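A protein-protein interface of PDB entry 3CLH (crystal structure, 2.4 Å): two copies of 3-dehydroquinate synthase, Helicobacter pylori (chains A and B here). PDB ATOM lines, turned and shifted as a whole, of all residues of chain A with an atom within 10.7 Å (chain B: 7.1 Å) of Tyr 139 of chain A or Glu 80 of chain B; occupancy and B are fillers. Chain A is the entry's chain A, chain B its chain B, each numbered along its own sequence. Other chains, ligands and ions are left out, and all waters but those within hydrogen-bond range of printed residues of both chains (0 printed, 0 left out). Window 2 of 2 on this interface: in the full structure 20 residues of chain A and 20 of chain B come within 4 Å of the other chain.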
ATOM      1  N   LYS A  66      10.629   7.522  11.715  1.00  0.00           N
ATOM      2  CA  LYS A  66      10.660   6.443  10.731  1.00  0.00           C
ATOM      3  C   LYS A  66      11.411   6.908   9.482  1.00  0.00           C
ATOM      4  O   LYS A  66      10.807   7.206   8.449  1.00  0.00           O
ATOM      5  CB  LYS A  66       9.236   5.991  10.388  1.00  0.00           C
ATOM      6  CG  LYS A  66       9.148   4.645   9.684  1.00  0.00           C
ATOM      7  CD  LYS A  66       7.710   4.303   9.336  1.00  0.00           C
ATOM      8  CE  LYS A  66       7.629   3.012   8.540  1.00  0.00           C
ATOM      9  NZ  LYS A  66       6.225   2.639   8.223  1.00  0.00           N
ATOM     10  N   ASN A  67      12.735   6.978   9.594  1.00  0.00           N
ATOM     11  CA  ASN A  67      13.592   7.458   8.509  1.00  0.00           C
ATOM     12  C   ASN A  67      14.926   6.709   8.435  1.00  0.00           C
ATOM     13  O   ASN A  67      15.079   5.646   9.041  1.00  0.00           O
ATOM     14  CB  ASN A  67      13.816   8.976   8.626  1.00  0.00           C
ATOM     15  CG  ASN A  67      14.228   9.410  10.029  1.00  0.00           C
ATOM     16  OD1 ASN A  67      15.055   8.770  10.680  1.00  0.00           O
ATOM     17  ND2 ASN A  67      13.654  10.514  10.493  1.00  0.00           N
ATOM     18  N   ILE A 135      10.985   2.450   5.336  1.00  0.00           N
ATOM     19  CA  ILE A 135      11.115   3.734   6.032  1.00  0.00           C
ATOM     20  C   ILE A 135      10.554   4.876   5.179  1.00  0.00           C
ATOM     21  O   ILE A 135      10.288   4.697   3.987  1.00  0.00           O
ATOM     22  CB  ILE A 135      12.592   4.046   6.408  1.00  0.00           C
ATOM     23  CG1 ILE A 135      13.515   3.894   5.189  1.00  0.00           C
ATOM     24  CG2 ILE A 135      13.051   3.165   7.571  1.00  0.00           C
ATOM     25  CD1 ILE A 135      14.837   4.636   5.303  1.00  0.00           C
ATOM     26  N   ASN A 136      10.377   6.043   5.796  1.00  0.00           N
ATOM     27  CA  ASN A 136       9.884   7.227   5.089  1.00  0.00           C
ATOM     28  C   ASN A 136      11.012   8.093   4.532  1.00  0.00           C
ATOM     29  O   ASN A 136      12.082   8.205   5.136  1.00  0.00           O
ATOM     30  CB  ASN A 136       8.974   8.069   5.992  1.00  0.00           C
ATOM     31  CG  ASN A 136       7.761   7.297   6.495  1.00  0.00           C
ATOM     32  OD1 ASN A 136       7.408   6.243   5.964  1.00  0.00           O
ATOM     33  ND2 ASN A 136       7.116   7.829   7.526  1.00  0.00           N
ATOM     34  N   THR A 137      10.754   8.701   3.377  1.00  0.00           N
ATOM     35  CA  THR A 137      11.713   9.578   2.706  1.00  0.00           C
ATOM     36  C   THR A 137      11.080  10.945   2.420  1.00  0.00           C
ATOM     37  O   THR A 137       9.852  11.068   2.442  1.00  0.00           O
ATOM     38  CB  THR A 137      12.225   8.949   1.385  1.00  0.00           C
ATOM     39  OG1 THR A 137      11.121   8.431   0.634  1.00  0.00           O
ATOM     40  CG2 THR A 137      13.216   7.829   1.670  1.00  0.00           C
ATOM     41  N   PRO A 138      11.910  11.983   2.164  1.00  0.00           N
ATOM     42  CA  PRO A 138      11.395  13.309   1.793  1.00  0.00           C
ATOM     43  C   PRO A 138      10.443  13.304   0.592  1.00  0.00           C
ATOM     44  O   PRO A 138       9.667  14.245   0.420  1.00  0.00           O
ATOM     45  CB  PRO A 138      12.665  14.091   1.449  1.00  0.00           C
ATOM     46  CG  PRO A 138      13.729  13.439   2.246  1.00  0.00           C
ATOM     47  CD  PRO A 138      13.384  11.981   2.242  1.00  0.00           C
ATOM     48  N   TYR A 139      10.509  12.251  -0.223  1.00  0.00           N
ATOM     49  CA  TYR A 139       9.640  12.107  -1.390  1.00  0.00           C
ATOM     50  C   TYR A 139       8.295  11.452  -1.058  1.00  0.00           C
ATOM     51  O   TYR A 139       7.346  11.544  -1.842  1.00  0.00           O
ATOM     52  CB  TYR A 139      10.355  11.331  -2.501  1.00  0.00           C
ATOM     53  CG  TYR A 139      11.496  12.091  -3.145  1.00  0.00           C
ATOM     54  CD1 TYR A 139      11.265  12.965  -4.207  1.00  0.00           C
ATOM     55  CD2 TYR A 139      12.806  11.937  -2.691  1.00  0.00           C
ATOM     56  CE1 TYR A 139      12.310  13.666  -4.803  1.00  0.00           C
ATOM     57  CE2 TYR A 139      13.859  12.633  -3.279  1.00  0.00           C
ATOM     58  CZ  TYR A 139      13.603  13.496  -4.334  1.00  0.00           C
ATOM     59  OH  TYR A 139      14.640  14.187  -4.920  1.00  0.00           O
ATOM     60  N   GLY A 140       8.217  10.798   0.101  1.00  0.00           N
ATOM     61  CA  GLY A 140       6.977  10.167   0.554  1.00  0.00           C
ATOM     62  C   GLY A 140       7.169   9.022   1.533  1.00  0.00           C
ATOM     63  O   GLY A 140       8.299   8.641   1.847  1.00  0.00           O
ATOM     64  N   LYS A 141       6.053   8.472   2.006  1.00  0.00           N
ATOM     65  CA  LYS A 141       6.062   7.397   2.999  1.00  0.00           C
ATOM     66  C   LYS A 141       6.158   6.012   2.366  1.00  0.00           C
ATOM     67  O   LYS A 141       5.550   5.753   1.324  1.00  0.00           O
ATOM     68  CB  LYS A 141       4.816   7.473   3.886  1.00  0.00           C
ATOM     69  CG  LYS A 141       4.802   8.641   4.860  1.00  0.00           C
ATOM     70  CD  LYS A 141       3.547   8.623   5.723  1.00  0.00           C
ATOM     71  CE  LYS A 141       3.566   9.727   6.770  1.00  0.00           C
ATOM     72  NZ  LYS A 141       3.436  11.088   6.175  1.00  0.00           N
ATOM     73  N   ASN A 142       6.927   5.135   3.013  1.00  0.00           N
ATOM     74  CA  ASN A 142       7.085   3.726   2.616  1.00  0.00           C
ATOM     75  C   ASN A 142       7.489   3.510   1.153  1.00  0.00           C
ATOM     76  O   ASN A 142       7.000   2.588   0.493  1.00  0.00           O
ATOM     77  CB  ASN A 142       5.823   2.917   2.962  1.00  0.00           C
ATOM     78  CG  ASN A 142       5.493   2.946   4.447  1.00  0.00           C
ATOM     79  OD1 ASN A 142       6.364   2.754   5.297  1.00  0.00           O
ATOM     80  ND2 ASN A 142       4.224   3.177   4.763  1.00  0.00           N
ATOM     81  N   LEU A 143       8.385   4.360   0.657  1.00  0.00           N
ATOM     82  CA  LEU A 143       8.860   4.265  -0.725  1.00  0.00           C
ATOM     83  C   LEU A 143      10.208   3.548  -0.826  1.00  0.00           C
ATOM     84  O   LEU A 143      10.594   3.089  -1.903  1.00  0.00           O
ATOM     85  CB  LEU A 143       8.925   5.651  -1.380  1.00  0.00           C
ATOM     86  CG  LEU A 143       7.622   6.451  -1.515  1.00  0.00           C
ATOM     87  CD1 LEU A 143       7.897   7.823  -2.110  1.00  0.00           C
ATOM     88  CD2 LEU A 143       6.572   5.717  -2.342  1.00  0.00           C
ATOM     89  N   ILE A 144      10.914   3.461   0.300  1.00  0.00           N
ATOM     90  CA  ILE A 144      12.159   2.699   0.387  1.00  0.00           C
ATOM     91  C   ILE A 144      11.999   1.574   1.408  1.00  0.00           C
ATOM     92  O   ILE A 144      11.893   1.824   2.611  1.00  0.00           O
ATOM     93  CB  ILE A 144      13.381   3.605   0.735  1.00  0.00           C
ATOM     94  CG1 ILE A 144      13.606   4.675  -0.346  1.00  0.00           C
ATOM     95  CG2 ILE A 144      14.648   2.768   0.964  1.00  0.00           C
ATOM     96  CD1 ILE A 144      13.892   4.139  -1.752  1.00  0.00           C
ATOM     97  N   HIS A 235      -5.951   8.654   1.903  1.00  0.00           N
ATOM     98  CA  HIS A 235      -4.679   9.285   1.547  1.00  0.00           C
ATOM     99  C   HIS A 235      -4.876  10.749   1.152  1.00  0.00           C
ATOM    100  O   HIS A 235      -4.029  11.596   1.443  1.00  0.00           O
ATOM    101  CB  HIS A 235      -3.993   8.507   0.417  1.00  0.00           C
ATOM    102  CG  HIS A 235      -2.741   9.152  -0.094  1.00  0.00           C
ATOM    103  ND1 HIS A 235      -1.530   9.044   0.553  1.00  0.00           N
ATOM    104  CD2 HIS A 235      -2.514   9.912  -1.192  1.00  0.00           C
ATOM    105  CE1 HIS A 235      -0.611   9.710  -0.123  1.00  0.00           C
ATOM    106  NE2 HIS A 235      -1.183  10.246  -1.186  1.00  0.00           N
ATOM    107  N   LYS A 239      -3.219  13.980   3.139  1.00  0.00           N
ATOM    108  CA  LYS A 239      -2.377  14.896   2.370  1.00  0.00           C
ATOM    109  C   LYS A 239      -2.886  16.336   2.455  1.00  0.00           C
ATOM    110  O   LYS A 239      -2.095  17.282   2.424  1.00  0.00           O
ATOM    111  CB  LYS A 239      -2.297  14.446   0.906  1.00  0.00           C
ATOM    112  CG  LYS A 239      -1.053  14.919   0.157  1.00  0.00           C
ATOM    113  CD  LYS A 239       0.173  14.080   0.509  1.00  0.00           C
ATOM    114  CE  LYS A 239       1.388  14.481  -0.315  1.00  0.00           C
ATOM    115  NZ  LYS A 239       1.261  14.089  -1.749  1.00  0.00           N
ATOM    116  N   TYR A 243      -1.042  15.311   7.524  1.00  0.00           N
ATOM    117  CA  TYR A 243      -0.813  14.264   8.535  1.00  0.00           C
ATOM    118  C   TYR A 243      -0.769  14.825   9.965  1.00  0.00           C
ATOM    119  O   TYR A 243       0.040  14.387  10.788  1.00  0.00           O
ATOM    120  CB  TYR A 243       0.472  13.473   8.232  1.00  0.00           C
ATOM    121  CG  TYR A 243       0.539  12.862   6.847  1.00  0.00           C
ATOM    122  CD1 TYR A 243       0.061  11.574   6.609  1.00  0.00           C
ATOM    123  CD2 TYR A 243       1.097  13.565   5.779  1.00  0.00           C
ATOM    124  CE1 TYR A 243       0.127  11.004   5.340  1.00  0.00           C
ATOM    125  CE2 TYR A 243       1.166  13.005   4.505  1.00  0.00           C
ATOM    126  CZ  TYR A 243       0.679  11.726   4.294  1.00  0.00           C
ATOM    127  OH  TYR A 243       0.746  11.168   3.038  1.00  0.00           O
ATOM    128  N   GLU B  53      11.129   7.303 -21.081  1.00  0.00           N
ATOM    129  CA  GLU B  53      11.990   8.418 -20.695  1.00  0.00           C
ATOM    130  C   GLU B  53      13.307   7.898 -20.128  1.00  0.00           C
ATOM    131  O   GLU B  53      13.317   7.042 -19.238  1.00  0.00           O
ATOM    132  CB  GLU B  53      11.286   9.322 -19.677  1.00  0.00           C
ATOM    133  CG  GLU B  53      11.967  10.670 -19.457  1.00  0.00           C
ATOM    134  CD  GLU B  53      11.316  11.502 -18.361  1.00  0.00           C
ATOM    135  OE1 GLU B  53      10.164  11.208 -17.976  1.00  0.00           O
ATOM    136  OE2 GLU B  53      11.962  12.459 -17.886  1.00  0.00           O
ATOM    137  N   ARG B  55      16.965   8.933 -18.375  1.00  0.00           N
ATOM    138  CA  ARG B  55      17.819   9.892 -17.673  1.00  0.00           C
ATOM    139  C   ARG B  55      19.075   9.208 -17.138  1.00  0.00           C
ATOM    140  O   ARG B  55      19.054   8.017 -16.819  1.00  0.00           O
ATOM    141  CB  ARG B  55      17.056  10.583 -16.539  1.00  0.00           C
ATOM    142  CG  ARG B  55      15.965  11.537 -17.005  1.00  0.00           C
ATOM    143  CD  ARG B  55      15.437  12.379 -15.857  1.00  0.00           C
ATOM    144  NE  ARG B  55      14.204  13.079 -16.213  1.00  0.00           N
ATOM    145  CZ  ARG B  55      13.514  13.867 -15.390  1.00  0.00           C
ATOM    146  NH1 ARG B  55      13.926  14.068 -14.144  1.00  0.00           N
ATOM    147  NH2 ARG B  55      12.405  14.455 -15.816  1.00  0.00           N
ATOM    148  N   GLU B  72      22.282   6.928  -2.237  1.00  0.00           N
ATOM    149  CA  GLU B  72      21.227   7.922  -2.048  1.00  0.00           C
ATOM    150  C   GLU B  72      21.004   8.733  -3.325  1.00  0.00           C
ATOM    151  O   GLU B  72      19.865   9.059  -3.663  1.00  0.00           O
ATOM    152  CB  GLU B  72      21.572   8.851  -0.879  1.00  0.00           C
ATOM    153  CG  GLU B  72      20.410   9.711  -0.383  1.00  0.00           C
ATOM    154  CD  GLU B  72      20.804  10.672   0.730  1.00  0.00           C
ATOM    155  OE1 GLU B  72      21.991  10.701   1.121  1.00  0.00           O
ATOM    156  OE2 GLU B  72      19.918  11.405   1.216  1.00  0.00           O
ATOM    157  N   LEU B  75      19.078   6.648  -5.829  1.00  0.00           N
ATOM    158  CA  LEU B  75      17.681   6.620  -5.393  1.00  0.00           C
ATOM    159  C   LEU B  75      16.975   7.951  -5.660  1.00  0.00           C
ATOM    160  O   LEU B  75      15.834   7.965  -6.124  1.00  0.00           O
ATOM    161  CB  LEU B  75      17.578   6.254  -3.908  1.00  0.00           C
ATOM    162  CG  LEU B  75      17.989   4.844  -3.466  1.00  0.00           C
ATOM    163  CD1 LEU B  75      18.184   4.802  -1.958  1.00  0.00           C
ATOM    164  CD2 LEU B  75      16.983   3.788  -3.913  1.00  0.00           C
ATOM    165  N   ASN B  76      17.661   9.056  -5.369  1.00  0.00           N
ATOM    166  CA  ASN B  76      17.118  10.398  -5.595  1.00  0.00           C
ATOM    167  C   ASN B  76      16.860  10.704  -7.069  1.00  0.00           C
ATOM    168  O   ASN B  76      15.858  11.339  -7.405  1.00  0.00           O
ATOM    169  CB  ASN B  76      18.025  11.471  -4.980  1.00  0.00           C
ATOM    170  CG  ASN B  76      17.922  11.532  -3.463  1.00  0.00           C
ATOM    171  OD1 ASN B  76      16.910  11.144  -2.874  1.00  0.00           O
ATOM    172  ND2 ASN B  76      18.974  12.030  -2.822  1.00  0.00           N
ATOM    173  N   ASN B  77      17.762  10.248  -7.938  1.00  0.00           N
ATOM    174  CA  ASN B  77      17.585  10.368  -9.387  1.00  0.00           C
ATOM    175  C   ASN B  77      16.390   9.565  -9.895  1.00  0.00           C
ATOM    176  O   ASN B  77      15.738   9.954 -10.867  1.00  0.00           O
ATOM    177  CB  ASN B  77      18.856   9.944 -10.132  1.00  0.00           C
ATOM    178  CG  ASN B  77      19.884  11.058 -10.219  1.00  0.00           C
ATOM    179  OD1 ASN B  77      20.144  11.589 -11.299  1.00  0.00           O
ATOM    180  ND2 ASN B  77      20.472  11.417  -9.084  1.00  0.00           N
ATOM    181  N   ALA B  78      16.116   8.444  -9.229  1.00  0.00           N
ATOM    182  CA  ALA B  78      14.954   7.616  -9.529  1.00  0.00           C
ATOM    183  C   ALA B  78      13.663   8.280  -9.047  1.00  0.00           C
ATOM    184  O   ALA B  78      12.612   8.133  -9.674  1.00  0.00           O
ATOM    185  CB  ALA B  78      15.112   6.239  -8.906  1.00  0.00           C
ATOM    186  N   PHE B  79      13.754   9.006  -7.933  1.00  0.00           N
ATOM    187  CA  PHE B  79      12.621   9.758  -7.392  1.00  0.00           C
ATOM    188  C   PHE B  79      12.327  11.024  -8.197  1.00  0.00           C
ATOM    189  O   PHE B  79      11.169  11.425  -8.325  1.00  0.00           O
ATOM    190  CB  PHE B  79      12.861  10.129  -5.923  1.00  0.00           C
ATOM    191  CG  PHE B  79      12.548   9.023  -4.948  1.00  0.00           C
ATOM    192  CD1 PHE B  79      11.256   8.517  -4.832  1.00  0.00           C
ATOM    193  CD2 PHE B  79      13.543   8.507  -4.122  1.00  0.00           C
ATOM    194  CE1 PHE B  79      10.966   7.501  -3.926  1.00  0.00           C
ATOM    195  CE2 PHE B  79      13.263   7.491  -3.213  1.00  0.00           C
ATOM    196  CZ  PHE B  79      11.971   6.988  -3.113  1.00  0.00           C
ATOM    197  N   GLU B  80      13.380  11.646  -8.729  1.00  0.00           N
ATOM    198  CA  GLU B  80      13.260  12.896  -9.487  1.00  0.00           C
ATOM    199  C   GLU B  80      12.525  12.732 -10.818  1.00  0.00           C
ATOM    200  O   GLU B  80      11.740  13.599 -11.206  1.00  0.00           O
ATOM    201  CB  GLU B  80      14.636  13.533  -9.716  1.00  0.00           C
ATOM    202  CG  GLU B  80      15.181  14.317  -8.522  1.00  0.00           C
ATOM    203  CD  GLU B  80      14.407  15.596  -8.238  1.00  0.00           C
ATOM    204  OE1 GLU B  80      14.105  16.345  -9.192  1.00  0.00           O
ATOM    205  OE2 GLU B  80      14.107  15.857  -7.054  1.00  0.00           O
ATOM    206  N   MET B  81      12.786  11.623 -11.508  1.00  0.00           N
ATOM    207  CA  MET B  81      12.104  11.318 -12.768  1.00  0.00           C
ATOM    208  C   MET B  81      10.831  10.494 -12.548  1.00  0.00           C
ATOM    209  O   MET B  81      10.185  10.063 -13.509  1.00  0.00           O
ATOM    210  CB  MET B  81      13.056  10.624 -13.754  1.00  0.00           C
ATOM    211  CG  MET B  81      13.517   9.230 -13.344  1.00  0.00           C
ATOM    212  SD  MET B  81      14.685   8.490 -14.508  1.00  0.00           S
ATOM    213  CE  MET B  81      13.676   8.310 -15.979  1.00  0.00           C
ATOM    214  N   GLN B  82      10.485  10.293 -11.276  1.00  0.00           N
ATOM    215  CA  GLN B  82       9.278   9.572 -10.851  1.00  0.00           C
ATOM    216  C   GLN B  82       9.200   8.141 -11.389  1.00  0.00           C
ATOM    217  O   GLN B  82       8.303   7.801 -12.166  1.00  0.00           O
ATOM    218  CB  GLN B  82       8.006  10.364 -11.193  1.00  0.00           C
ATOM    219  CG  GLN B  82       7.825  11.643 -10.384  1.00  0.00           C
ATOM    220  CD  GLN B  82       6.538  12.378 -10.713  1.00  0.00           C
ATOM    221  OE1 GLN B  82       6.098  12.411 -11.865  1.00  0.00           O
ATOM    222  NE2 GLN B  82       5.930  12.984  -9.700  1.00  0.00           N
ATOM    223  N   LEU B  83      10.153   7.311 -10.970  1.00  0.00           N
ATOM    224  CA  LEU B  83      10.139   5.892 -11.307  1.00  0.00           C
ATOM    225  C   LEU B  83       9.225   5.133 -10.351  1.00  0.00           C
ATOM    226  O   LEU B  83       9.156   5.449  -9.161  1.00  0.00           O
ATOM    227  CB  LEU B  83      11.554   5.300 -11.272  1.00  0.00           C
ATOM    228  CG  LEU B  83      12.614   5.763 -12.281  1.00  0.00           C
ATOM    229  CD1 LEU B  83      13.875   4.926 -12.133  1.00  0.00           C
ATOM    230  CD2 LEU B  83      12.111   5.704 -13.718  1.00  0.00           C
ATOM    231  N   TYR B 108      14.207   0.303  -3.821  1.00  0.00           N
ATOM    232  CA  TYR B 108      13.345   1.321  -4.419  1.00  0.00           C
ATOM    233  C   TYR B 108      11.970   0.733  -4.733  1.00  0.00           C
ATOM    234  O   TYR B 108      11.859  -0.211  -5.521  1.00  0.00           O
ATOM    235  CB  TYR B 108      13.993   1.895  -5.683  1.00  0.00           C
ATOM    236  CG  TYR B 108      13.277   3.093  -6.265  1.00  0.00           C
ATOM    237  CD1 TYR B 108      13.421   4.359  -5.697  1.00  0.00           C
ATOM    238  CD2 TYR B 108      12.465   2.963  -7.389  1.00  0.00           C
ATOM    239  CE1 TYR B 108      12.766   5.464  -6.230  1.00  0.00           C
ATOM    240  CE2 TYR B 108      11.808   4.061  -7.930  1.00  0.00           C
ATOM    241  CZ  TYR B 108      11.961   5.308  -7.346  1.00  0.00           C
ATOM    242  OH  TYR B 108      11.313   6.399  -7.877  1.00  0.00           O
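OH of Tyr 139 of chain A sits at hydrogen-bond distance from OE2 of Glu 80 of chain B.
N of Ile 135 of chain A lies within hydrogen-bond range of O of Ile 144 of chain A (2.9 Å). The backbone carbonyl oxygen (O) of Glu 72 of chain B sits close to the side-chain amide nitrogen (ND2) of Asn 76 of chain B. O of Ala 78 of chain B lies within hydrogen-bond range of OH of Tyr 108 of chain B, at 2.8 Å. The backbone carbonyl oxygen (O) of Leu 83 of chain B is in hydrogen-bond range of the side-chain hydroxyl (OH) of Tyr 108 of chain B (2.7 Å).
Among the printed residues, merely in contact across the chains: Tyr 139 of chain A with Asn 76 of chain B, Leu 143 of chain A with Phe 79 of chain B, Tyr 139 of chain A with Phe 79 of chain B, Ile 144 of chain A with Phe 79 of chain B, Ile 144 of chain A with Leu 75 of chain B, Ile 144 of chain A with Tyr 108 of chain B and Leu 143 of chain A with Tyr 108 of chain B.
Tyr 139 of chain A touches three residues of chain B. Of the printed residues of chain A, Glu 80 of chain B touches Tyr 139 (2.8 Å). Of chain A, only Tyr 139 (3.4 Å) comes within 4 Å of Asn 76 of chain B. No residue of chain A comes within 4 Å of Asn 77 of chain B. No residue of chain A comes within 4 Å of Ala 78 of chain B. Of chain A, only Tyr 139, Leu 143 and Ile 144 come within 4 Å of Phe 79 of chain B. No residue of chain A comes within 4 Å of Gln 82 of chain B. Of the printed residues of chain A, Leu 75 of chain B touches Ile 144. Of the printed residues of chain B, Leu 143 of chain A touches Phe 79 and Tyr 108. Of the printed residues of chain B, Ile 144 of chain A touches Leu 75 (3.8 Å), Phe 79 (3.7 Å) and Tyr 108 (3.9 Å). Of the printed residues of chain A, Tyr 108 of chain B touches Leu 143 and Ile 144. Arg 55 of chain B touches none of the printed residues of chain A. Gly 140 of chain A touches none of the printed residues of chain B. The nearest residue of chain A that does not touch Glu 80 of chain B is Pro 138 of chain A (8.8 Å).
Of the 15 printed residues of chain A, 3 touch a printed residue of chain B. Hydrophobic or aromatic side chains of chain A that line the printed part of chain B: Tyr 139, Leu 143 and Ile 144. Of the 13 printed residues of chain B, 5 touch a printed residue of chain A. Among the printed residues, no Asp or Glu carboxylate lies within 4 Å of a Lys or Arg side-chain nitrogen of the other chain.
No position is printed for both chains.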
